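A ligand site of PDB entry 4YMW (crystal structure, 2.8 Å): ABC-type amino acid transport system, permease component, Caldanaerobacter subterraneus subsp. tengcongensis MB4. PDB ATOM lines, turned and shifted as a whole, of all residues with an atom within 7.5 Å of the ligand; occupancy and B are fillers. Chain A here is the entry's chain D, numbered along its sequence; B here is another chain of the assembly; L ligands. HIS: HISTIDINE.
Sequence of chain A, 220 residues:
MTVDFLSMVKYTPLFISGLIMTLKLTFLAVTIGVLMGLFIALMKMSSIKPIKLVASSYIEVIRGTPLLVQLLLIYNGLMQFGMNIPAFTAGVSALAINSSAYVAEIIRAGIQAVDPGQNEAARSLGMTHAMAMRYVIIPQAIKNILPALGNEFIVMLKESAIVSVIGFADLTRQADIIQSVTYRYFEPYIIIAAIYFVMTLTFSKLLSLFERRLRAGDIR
The side-chain sulfur of Met 156 lies within hydrogen-bond range of a nitrogen (NE2) of the ligand, at 3.6 Å.
A nitrogen (NE2) of the ligand sits close to the side-chain carboxylate of Glu 152.
OE2 of Glu 159 of chain A is in salt-bridge range of N of the ligand.
The side-chain amide nitrogen (NE2) of Gln 70 sits close to the side-chain amide nitrogen (ND2) of Asn 98 (3.1 Å).
OE1 of Glu 152 sits at hydrogen-bond distance from OG of Ser 99, at 3.4 Å.
The side-chain amino group (NZ) of Lys 158 of chain B is in hydrogen-bond range of the side-chain hydroxyl (OH) of Tyr 102, at 2.8 Å.
The side-chain amino group (NZ) of Lys 158 of chain B is in hydrogen-bond range of the backbone carbonyl oxygen (O) of Arg 63 (2.4 Å).
The backbone carbonyl oxygen (O) of Arg 63 lies within hydrogen-bond range of the side-chain hydroxyl (OH) of Tyr 102, at 3.3 Å.
Residues that only touch the ligand: Asn 98 (2.9 Å), Tyr 102 (3.1 Å), Lys 158 of chain B (3.8 Å), Glu 159 of chain B (3.8 Å) and Leu 67 (3.96 Å).
Within 4 Å of the ligand: Leu 67, Asn 98, Tyr 102, Glu 152, Met 156, Glu 159 of chain A, Lys 158 of chain B and Glu 159 of chain B.
The nearest printed residue that does not touch the ligand is Val 155 of chain A (4.6 Å).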
ATOM      1  N   ILE A  62      -0.617  -2.854  21.206  1.00  0.00           N
ATOM      2  CA  ILE A  62      -1.290  -2.790  19.915  1.00  0.00           C
ATOM      3  C   ILE A  62      -2.570  -1.955  19.917  1.00  0.00           C
ATOM      4  O   ILE A  62      -2.861  -1.271  18.936  1.00  0.00           O
ATOM      5  CB  ILE A  62      -1.628  -4.181  19.434  1.00  0.00           C
ATOM      6  CG1 ILE A  62      -0.348  -4.873  19.027  1.00  0.00           C
ATOM      7  CG2 ILE A  62      -2.559  -4.137  18.228  1.00  0.00           C
ATOM      8  CD1 ILE A  62      -0.583  -6.234  18.613  1.00  0.00           C
ATOM      9  N   ARG A  63      -3.368  -1.977  20.978  1.00  0.00           N
ATOM     10  CA  ARG A  63      -4.604  -1.208  20.909  1.00  0.00           C
ATOM     11  C   ARG A  63      -4.345   0.274  21.162  1.00  0.00           C
ATOM     12  O   ARG A  63      -5.067   1.122  20.648  1.00  0.00           O
ATOM     13  CB  ARG A  63      -5.640  -1.744  21.919  1.00  0.00           C
ATOM     14  CG  ARG A  63      -5.913  -3.260  21.824  1.00  0.00           C
ATOM     15  CD  ARG A  63      -7.067  -3.699  22.751  1.00  0.00           C
ATOM     16  NE  ARG A  63      -8.347  -3.087  22.424  1.00  0.00           N
ATOM     17  CZ  ARG A  63      -9.139  -2.487  23.314  1.00  0.00           C
ATOM     18  NH1 ARG A  63      -8.754  -2.413  24.583  1.00  0.00           N
ATOM     19  NH2 ARG A  63     -10.303  -1.960  22.937  1.00  0.00           N
ATOM     20  N   THR A  65      -1.866   2.099  20.108  1.00  0.00           N
ATOM     21  CA  THR A  65      -0.918   2.547  19.093  1.00  0.00           C
ATOM     22  C   THR A  65      -1.579   2.455  17.737  1.00  0.00           C
ATOM     23  O   THR A  65      -2.302   1.492  17.464  1.00  0.00           O
ATOM     24  CB  THR A  65       0.352   1.691  19.139  1.00  0.00           C
ATOM     25  OG1 THR A  65       1.374   2.379  19.872  1.00  0.00           O
ATOM     26  CG2 THR A  65       0.851   1.344  17.769  1.00  0.00           C
ATOM     27  N   PRO A  66      -1.364   3.469  16.873  1.00  0.00           N
ATOM     28  CA  PRO A  66      -2.120   3.590  15.618  1.00  0.00           C
ATOM     29  C   PRO A  66      -1.917   2.409  14.681  1.00  0.00           C
ATOM     30  O   PRO A  66      -0.880   1.747  14.743  1.00  0.00           O
ATOM     31  CB  PRO A  66      -1.582   4.879  15.010  1.00  0.00           C
ATOM     32  CG  PRO A  66      -1.066   5.665  16.180  1.00  0.00           C
ATOM     33  CD  PRO A  66      -0.497   4.636  17.109  1.00  0.00           C
ATOM     34  N   LEU A  67      -2.912   2.110  13.849  1.00  0.00           N
ATOM     35  CA  LEU A  67      -2.733   1.029  12.890  1.00  0.00           C
ATOM     36  C   LEU A  67      -1.673   1.405  11.850  1.00  0.00           C
ATOM     37  O   LEU A  67      -0.881   0.559  11.426  1.00  0.00           O
ATOM     38  CB  LEU A  67      -4.052   0.671  12.206  1.00  0.00           C
ATOM     39  CG  LEU A  67      -3.964  -0.300  11.033  1.00  0.00           C
ATOM     40  CD1 LEU A  67      -3.295  -1.583  11.426  1.00  0.00           C
ATOM     41  CD2 LEU A  67      -5.355  -0.565  10.498  1.00  0.00           C
ATOM     42  N   LEU A  68      -1.648   2.679  11.479  1.00  0.00           N
ATOM     43  CA  LEU A  68      -0.750   3.154  10.434  1.00  0.00           C
ATOM     44  C   LEU A  68       0.707   2.908  10.819  1.00  0.00           C
ATOM     45  O   LEU A  68       1.466   2.311  10.025  1.00  0.00           O
ATOM     46  CB  LEU A  68      -0.984   4.630  10.165  1.00  0.00           C
ATOM     47  CG  LEU A  68      -0.061   5.242   9.121  1.00  0.00           C
ATOM     48  CD1 LEU A  68      -0.239   4.514   7.821  1.00  0.00           C
ATOM     49  CD2 LEU A  68      -0.345   6.717   8.923  1.00  0.00           C
ATOM     50  N   GLN A  70       1.864   0.736  12.824  1.00  0.00           N
ATOM     51  CA  GLN A  70       2.175  -0.701  12.807  1.00  0.00           C
ATOM     52  C   GLN A  70       2.414  -1.209  11.375  1.00  0.00           C
ATOM     53  O   GLN A  70       3.324  -2.026  11.148  1.00  0.00           O
ATOM     54  CB  GLN A  70       1.063  -1.526  13.477  1.00  0.00           C
ATOM     55  CG  GLN A  70       0.878  -1.214  14.960  1.00  0.00           C
ATOM     56  CD  GLN A  70      -0.499  -1.598  15.516  1.00  0.00           C
ATOM     57  OE1 GLN A  70      -1.075  -0.847  16.298  1.00  0.00           O
ATOM     58  NE2 GLN A  70      -1.025  -2.745  15.098  1.00  0.00           N
ATOM     59  N   LEU A  95      -2.695  -5.897   9.683  1.00  0.00           N
ATOM     60  CA  LEU A  95      -4.107  -6.028  10.012  1.00  0.00           C
ATOM     61  C   LEU A  95      -4.380  -7.234  10.906  1.00  0.00           C
ATOM     62  O   LEU A  95      -5.021  -7.104  11.935  1.00  0.00           O
ATOM     63  CB  LEU A  95      -4.952  -6.092   8.738  1.00  0.00           C
ATOM     64  CG  LEU A  95      -5.109  -4.796   7.925  1.00  0.00           C
ATOM     65  CD1 LEU A  95      -6.192  -4.948   6.885  1.00  0.00           C
ATOM     66  CD2 LEU A  95      -5.388  -3.590   8.812  1.00  0.00           C
ATOM     67  N   ASN A  98      -3.150  -6.434  14.510  1.00  0.00           N
ATOM     68  CA  ASN A  98      -4.039  -5.435  15.114  1.00  0.00           C
ATOM     69  C   ASN A  98      -5.417  -6.033  15.537  1.00  0.00           C
ATOM     70  O   ASN A  98      -5.875  -5.952  16.711  1.00  0.00           O
ATOM     71  CB  ASN A  98      -4.219  -4.294  14.110  1.00  0.00           C
ATOM     72  CG  ASN A  98      -4.829  -3.061  14.718  1.00  0.00           C
ATOM     73  OD1 ASN A  98      -5.956  -2.707  14.394  1.00  0.00           O
ATOM     74  ND2 ASN A  98      -4.072  -2.354  15.546  1.00  0.00           N
ATOM     75  N   SER A  99      -6.045  -6.663  14.557  1.00  0.00           N
ATOM     76  CA  SER A  99      -7.258  -7.443  14.732  1.00  0.00           C
ATOM     77  C   SER A  99      -7.072  -8.546  15.766  1.00  0.00           C
ATOM     78  O   SER A  99      -7.988  -8.863  16.482  1.00  0.00           O
ATOM     79  CB  SER A  99      -7.691  -8.051  13.392  1.00  0.00           C
ATOM     80  OG  SER A  99      -8.830  -8.860  13.522  1.00  0.00           O
ATOM     81  N   SER A 100      -5.875  -9.130  15.849  1.00  0.00           N
ATOM     82  CA  SER A 100      -5.658 -10.161  16.845  1.00  0.00           C
ATOM     83  C   SER A 100      -5.844  -9.581  18.234  1.00  0.00           C
ATOM     84  O   SER A 100      -6.465 -10.201  19.088  1.00  0.00           O
ATOM     85  CB  SER A 100      -4.258 -10.760  16.739  1.00  0.00           C
ATOM     86  OG  SER A 100      -3.311  -9.975  17.450  1.00  0.00           O
ATOM     87  N   ALA A 101      -5.319  -8.376  18.480  1.00  0.00           N
ATOM     88  CA  ALA A 101      -5.560  -7.771  19.815  1.00  0.00           C
ATOM     89  C   ALA A 101      -7.052  -7.482  20.075  1.00  0.00           C
ATOM     90  O   ALA A 101      -7.623  -7.883  21.132  1.00  0.00           O
ATOM     91  CB  ALA A 101      -4.755  -6.492  19.969  1.00  0.00           C
ATOM     92  N   TYR A 102      -7.675  -6.764  19.139  1.00  0.00           N
ATOM     93  CA  TYR A 102      -9.078  -6.402  19.354  1.00  0.00           C
ATOM     94  C   TYR A 102      -9.994  -7.651  19.517  1.00  0.00           C
ATOM     95  O   TYR A 102     -11.013  -7.598  20.223  1.00  0.00           O
ATOM     96  CB  TYR A 102      -9.583  -5.486  18.237  1.00  0.00           C
ATOM     97  CG  TYR A 102      -9.004  -4.093  18.358  1.00  0.00           C
ATOM     98  CD1 TYR A 102      -9.698  -3.082  19.006  1.00  0.00           C
ATOM     99  CD2 TYR A 102      -7.730  -3.814  17.875  1.00  0.00           C
ATOM    100  CE1 TYR A 102      -9.156  -1.808  19.141  1.00  0.00           C
ATOM    101  CE2 TYR A 102      -7.185  -2.537  17.993  1.00  0.00           C
ATOM    102  CZ  TYR A 102      -7.897  -1.538  18.619  1.00  0.00           C
ATOM    103  OH  TYR A 102      -7.344  -0.281  18.741  1.00  0.00           O
ATOM    104  N   VAL A 103      -9.625  -8.754  18.866  1.00  0.00           N
ATOM    105  CA  VAL A 103     -10.308 -10.038  19.039  1.00  0.00           C
ATOM    106  C   VAL A 103     -10.028 -10.656  20.417  1.00  0.00           C
ATOM    107  O   VAL A 103     -10.945 -11.174  21.048  1.00  0.00           O
ATOM    108  CB  VAL A 103      -9.922 -11.043  17.935  1.00  0.00           C
ATOM    109  CG1 VAL A 103     -10.041 -12.471  18.414  1.00  0.00           C
ATOM    110  CG2 VAL A 103     -10.778 -10.821  16.694  1.00  0.00           C
ATOM    111  N   GLU A 152     -16.540  -6.816  13.934  1.00  0.00           N
ATOM    112  CA  GLU A 152     -15.117  -6.593  13.785  1.00  0.00           C
ATOM    113  C   GLU A 152     -14.717  -6.651  12.334  1.00  0.00           C
ATOM    114  O   GLU A 152     -14.012  -5.772  11.846  1.00  0.00           O
ATOM    115  CB  GLU A 152     -14.323  -7.624  14.570  1.00  0.00           C
ATOM    116  CG  GLU A 152     -13.387  -6.987  15.544  1.00  0.00           C
ATOM    117  CD  GLU A 152     -12.272  -6.284  14.855  1.00  0.00           C
ATOM    118  OE1 GLU A 152     -11.589  -6.940  14.046  1.00  0.00           O
ATOM    119  OE2 GLU A 152     -12.082  -5.073  15.135  1.00  0.00           O
ATOM    120  N   VAL A 155     -15.753  -3.479  10.685  1.00  0.00           N
ATOM    121  CA  VAL A 155     -14.836  -2.364  10.924  1.00  0.00           C
ATOM    122  C   VAL A 155     -13.536  -2.531  10.132  1.00  0.00           C
ATOM    123  O   VAL A 155     -12.963  -1.556   9.629  1.00  0.00           O
ATOM    124  CB  VAL A 155     -14.522  -2.212  12.421  1.00  0.00           C
ATOM    125  CG1 VAL A 155     -13.478  -1.130  12.642  1.00  0.00           C
ATOM    126  CG2 VAL A 155     -15.766  -1.890  13.178  1.00  0.00           C
ATOM    127  N   MET A 156     -13.074  -3.770  10.019  1.00  0.00           N
ATOM    128  CA  MET A 156     -11.857  -4.070   9.286  1.00  0.00           C
ATOM    129  C   MET A 156     -11.953  -3.748   7.808  1.00  0.00           C
ATOM    130  O   MET A 156     -10.943  -3.368   7.205  1.00  0.00           O
ATOM    131  CB  MET A 156     -11.446  -5.519   9.477  1.00  0.00           C
ATOM    132  CG  MET A 156     -10.796  -5.720  10.808  1.00  0.00           C
ATOM    133  SD  MET A 156      -9.562  -4.422  11.076  1.00  0.00           S
ATOM    134  CE  MET A 156      -8.103  -5.223  10.409  1.00  0.00           C
ATOM    135  N   GLU A 159     -11.146  -0.196   7.771  1.00  0.00           N
ATOM    136  CA  GLU A 159      -9.790   0.040   8.210  1.00  0.00           C
ATOM    137  C   GLU A 159      -8.751  -0.325   7.151  1.00  0.00           C
ATOM    138  O   GLU A 159      -7.719   0.353   7.043  1.00  0.00           O
ATOM    139  CB  GLU A 159      -9.534  -0.718   9.517  1.00  0.00           C
ATOM    140  CG  GLU A 159     -10.191  -0.037  10.702  1.00  0.00           C
ATOM    141  CD  GLU A 159      -9.533   1.281  11.042  1.00  0.00           C
ATOM    142  OE1 GLU A 159      -8.344   1.453  10.734  1.00  0.00           O
ATOM    143  OE2 GLU A 159     -10.217   2.164  11.612  1.00  0.00           O
ATOM    144  N   ILE A 162      -6.313   1.523   4.400  1.00  0.00           N
ATOM    145  CA  ILE A 162      -5.064   2.190   4.727  1.00  0.00           C
ATOM    146  C   ILE A 162      -3.854   1.535   4.073  1.00  0.00           C
ATOM    147  O   ILE A 162      -2.772   2.099   4.086  1.00  0.00           O
ATOM    148  CB  ILE A 162      -4.830   2.223   6.245  1.00  0.00           C
ATOM    149  CG1 ILE A 162      -3.942   3.405   6.597  1.00  0.00           C
ATOM    150  CG2 ILE A 162      -4.205   0.925   6.726  1.00  0.00           C
ATOM    151  CD1 ILE A 162      -3.455   3.359   7.991  1.00  0.00           C
ATOM    152  N   VAL B 155      -9.353   8.220  21.087  1.00  0.00           N
ATOM    153  CA  VAL B 155      -9.304   7.478  19.817  1.00  0.00           C
ATOM    154  C   VAL B 155      -8.794   8.355  18.642  1.00  0.00           C
ATOM    155  O   VAL B 155      -8.042   7.893  17.764  1.00  0.00           O
ATOM    156  CB  VAL B 155     -10.675   6.870  19.488  1.00  0.00           C
ATOM    157  CG1 VAL B 155     -10.663   6.140  18.158  1.00  0.00           C
ATOM    158  CG2 VAL B 155     -11.080   5.913  20.579  1.00  0.00           C
ATOM    159  N   LYS B 158      -4.987   8.457  18.090  1.00  0.00           N
ATOM    160  CA  LYS B 158      -4.477   7.401  17.224  1.00  0.00           C
ATOM    161  C   LYS B 158      -4.850   7.632  15.759  1.00  0.00           C
ATOM    162  O   LYS B 158      -4.039   7.408  14.853  1.00  0.00           O
ATOM    163  CB  LYS B 158      -4.983   6.019  17.645  1.00  0.00           C
ATOM    164  CG  LYS B 158      -4.425   5.541  18.954  1.00  0.00           C
ATOM    165  CD  LYS B 158      -4.710   4.056  19.121  1.00  0.00           C
ATOM    166  CE  LYS B 158      -6.192   3.773  19.226  1.00  0.00           C
ATOM    167  NZ  LYS B 158      -6.456   2.316  19.047  1.00  0.00           N
ATOM    168  N   GLU B 159      -6.093   8.076  15.538  1.00  0.00           N
ATOM    169  CA  GLU B 159      -6.605   8.278  14.190  1.00  0.00           C
ATOM    170  C   GLU B 159      -5.868   9.361  13.391  1.00  0.00           C
ATOM    171  O   GLU B 159      -5.687   9.238  12.173  1.00  0.00           O
ATOM    172  CB  GLU B 159      -8.102   8.606  14.261  1.00  0.00           C
ATOM    173  CG  GLU B 159      -8.996   7.404  14.493  1.00  0.00           C
ATOM    174  CD  GLU B 159      -9.077   6.512  13.275  1.00  0.00           C
ATOM    175  OE1 GLU B 159      -8.849   7.009  12.166  1.00  0.00           O
ATOM    176  OE2 GLU B 159      -9.379   5.312  13.409  1.00  0.00           O
HETATM  177  N   HIS L   1      -9.219   1.272  13.993  1.00  0.00           N
HETATM  178  CA  HIS L   1      -8.448   1.112  15.214  1.00  0.00           C
HETATM  179  C   HIS L   1      -7.422   2.229  15.374  1.00  0.00           C
HETATM  180  O   HIS L   1      -6.794   2.658  14.409  1.00  0.00           O
HETATM  181  CB  HIS L   1      -7.747  -0.246  15.210  1.00  0.00           C
HETATM  182  CG  HIS L   1      -8.667  -1.408  15.058  1.00  0.00           C
HETATM  183  ND1 HIS L   1      -9.590  -1.779  16.023  1.00  0.00           N
HETATM  184  CD2 HIS L   1      -8.790  -2.336  14.066  1.00  0.00           C
HETATM  185  CE1 HIS L   1     -10.243  -2.846  15.623  1.00  0.00           C
HETATM  186  NE2 HIS L   1      -9.784  -3.214  14.440  1.00  0.00           N
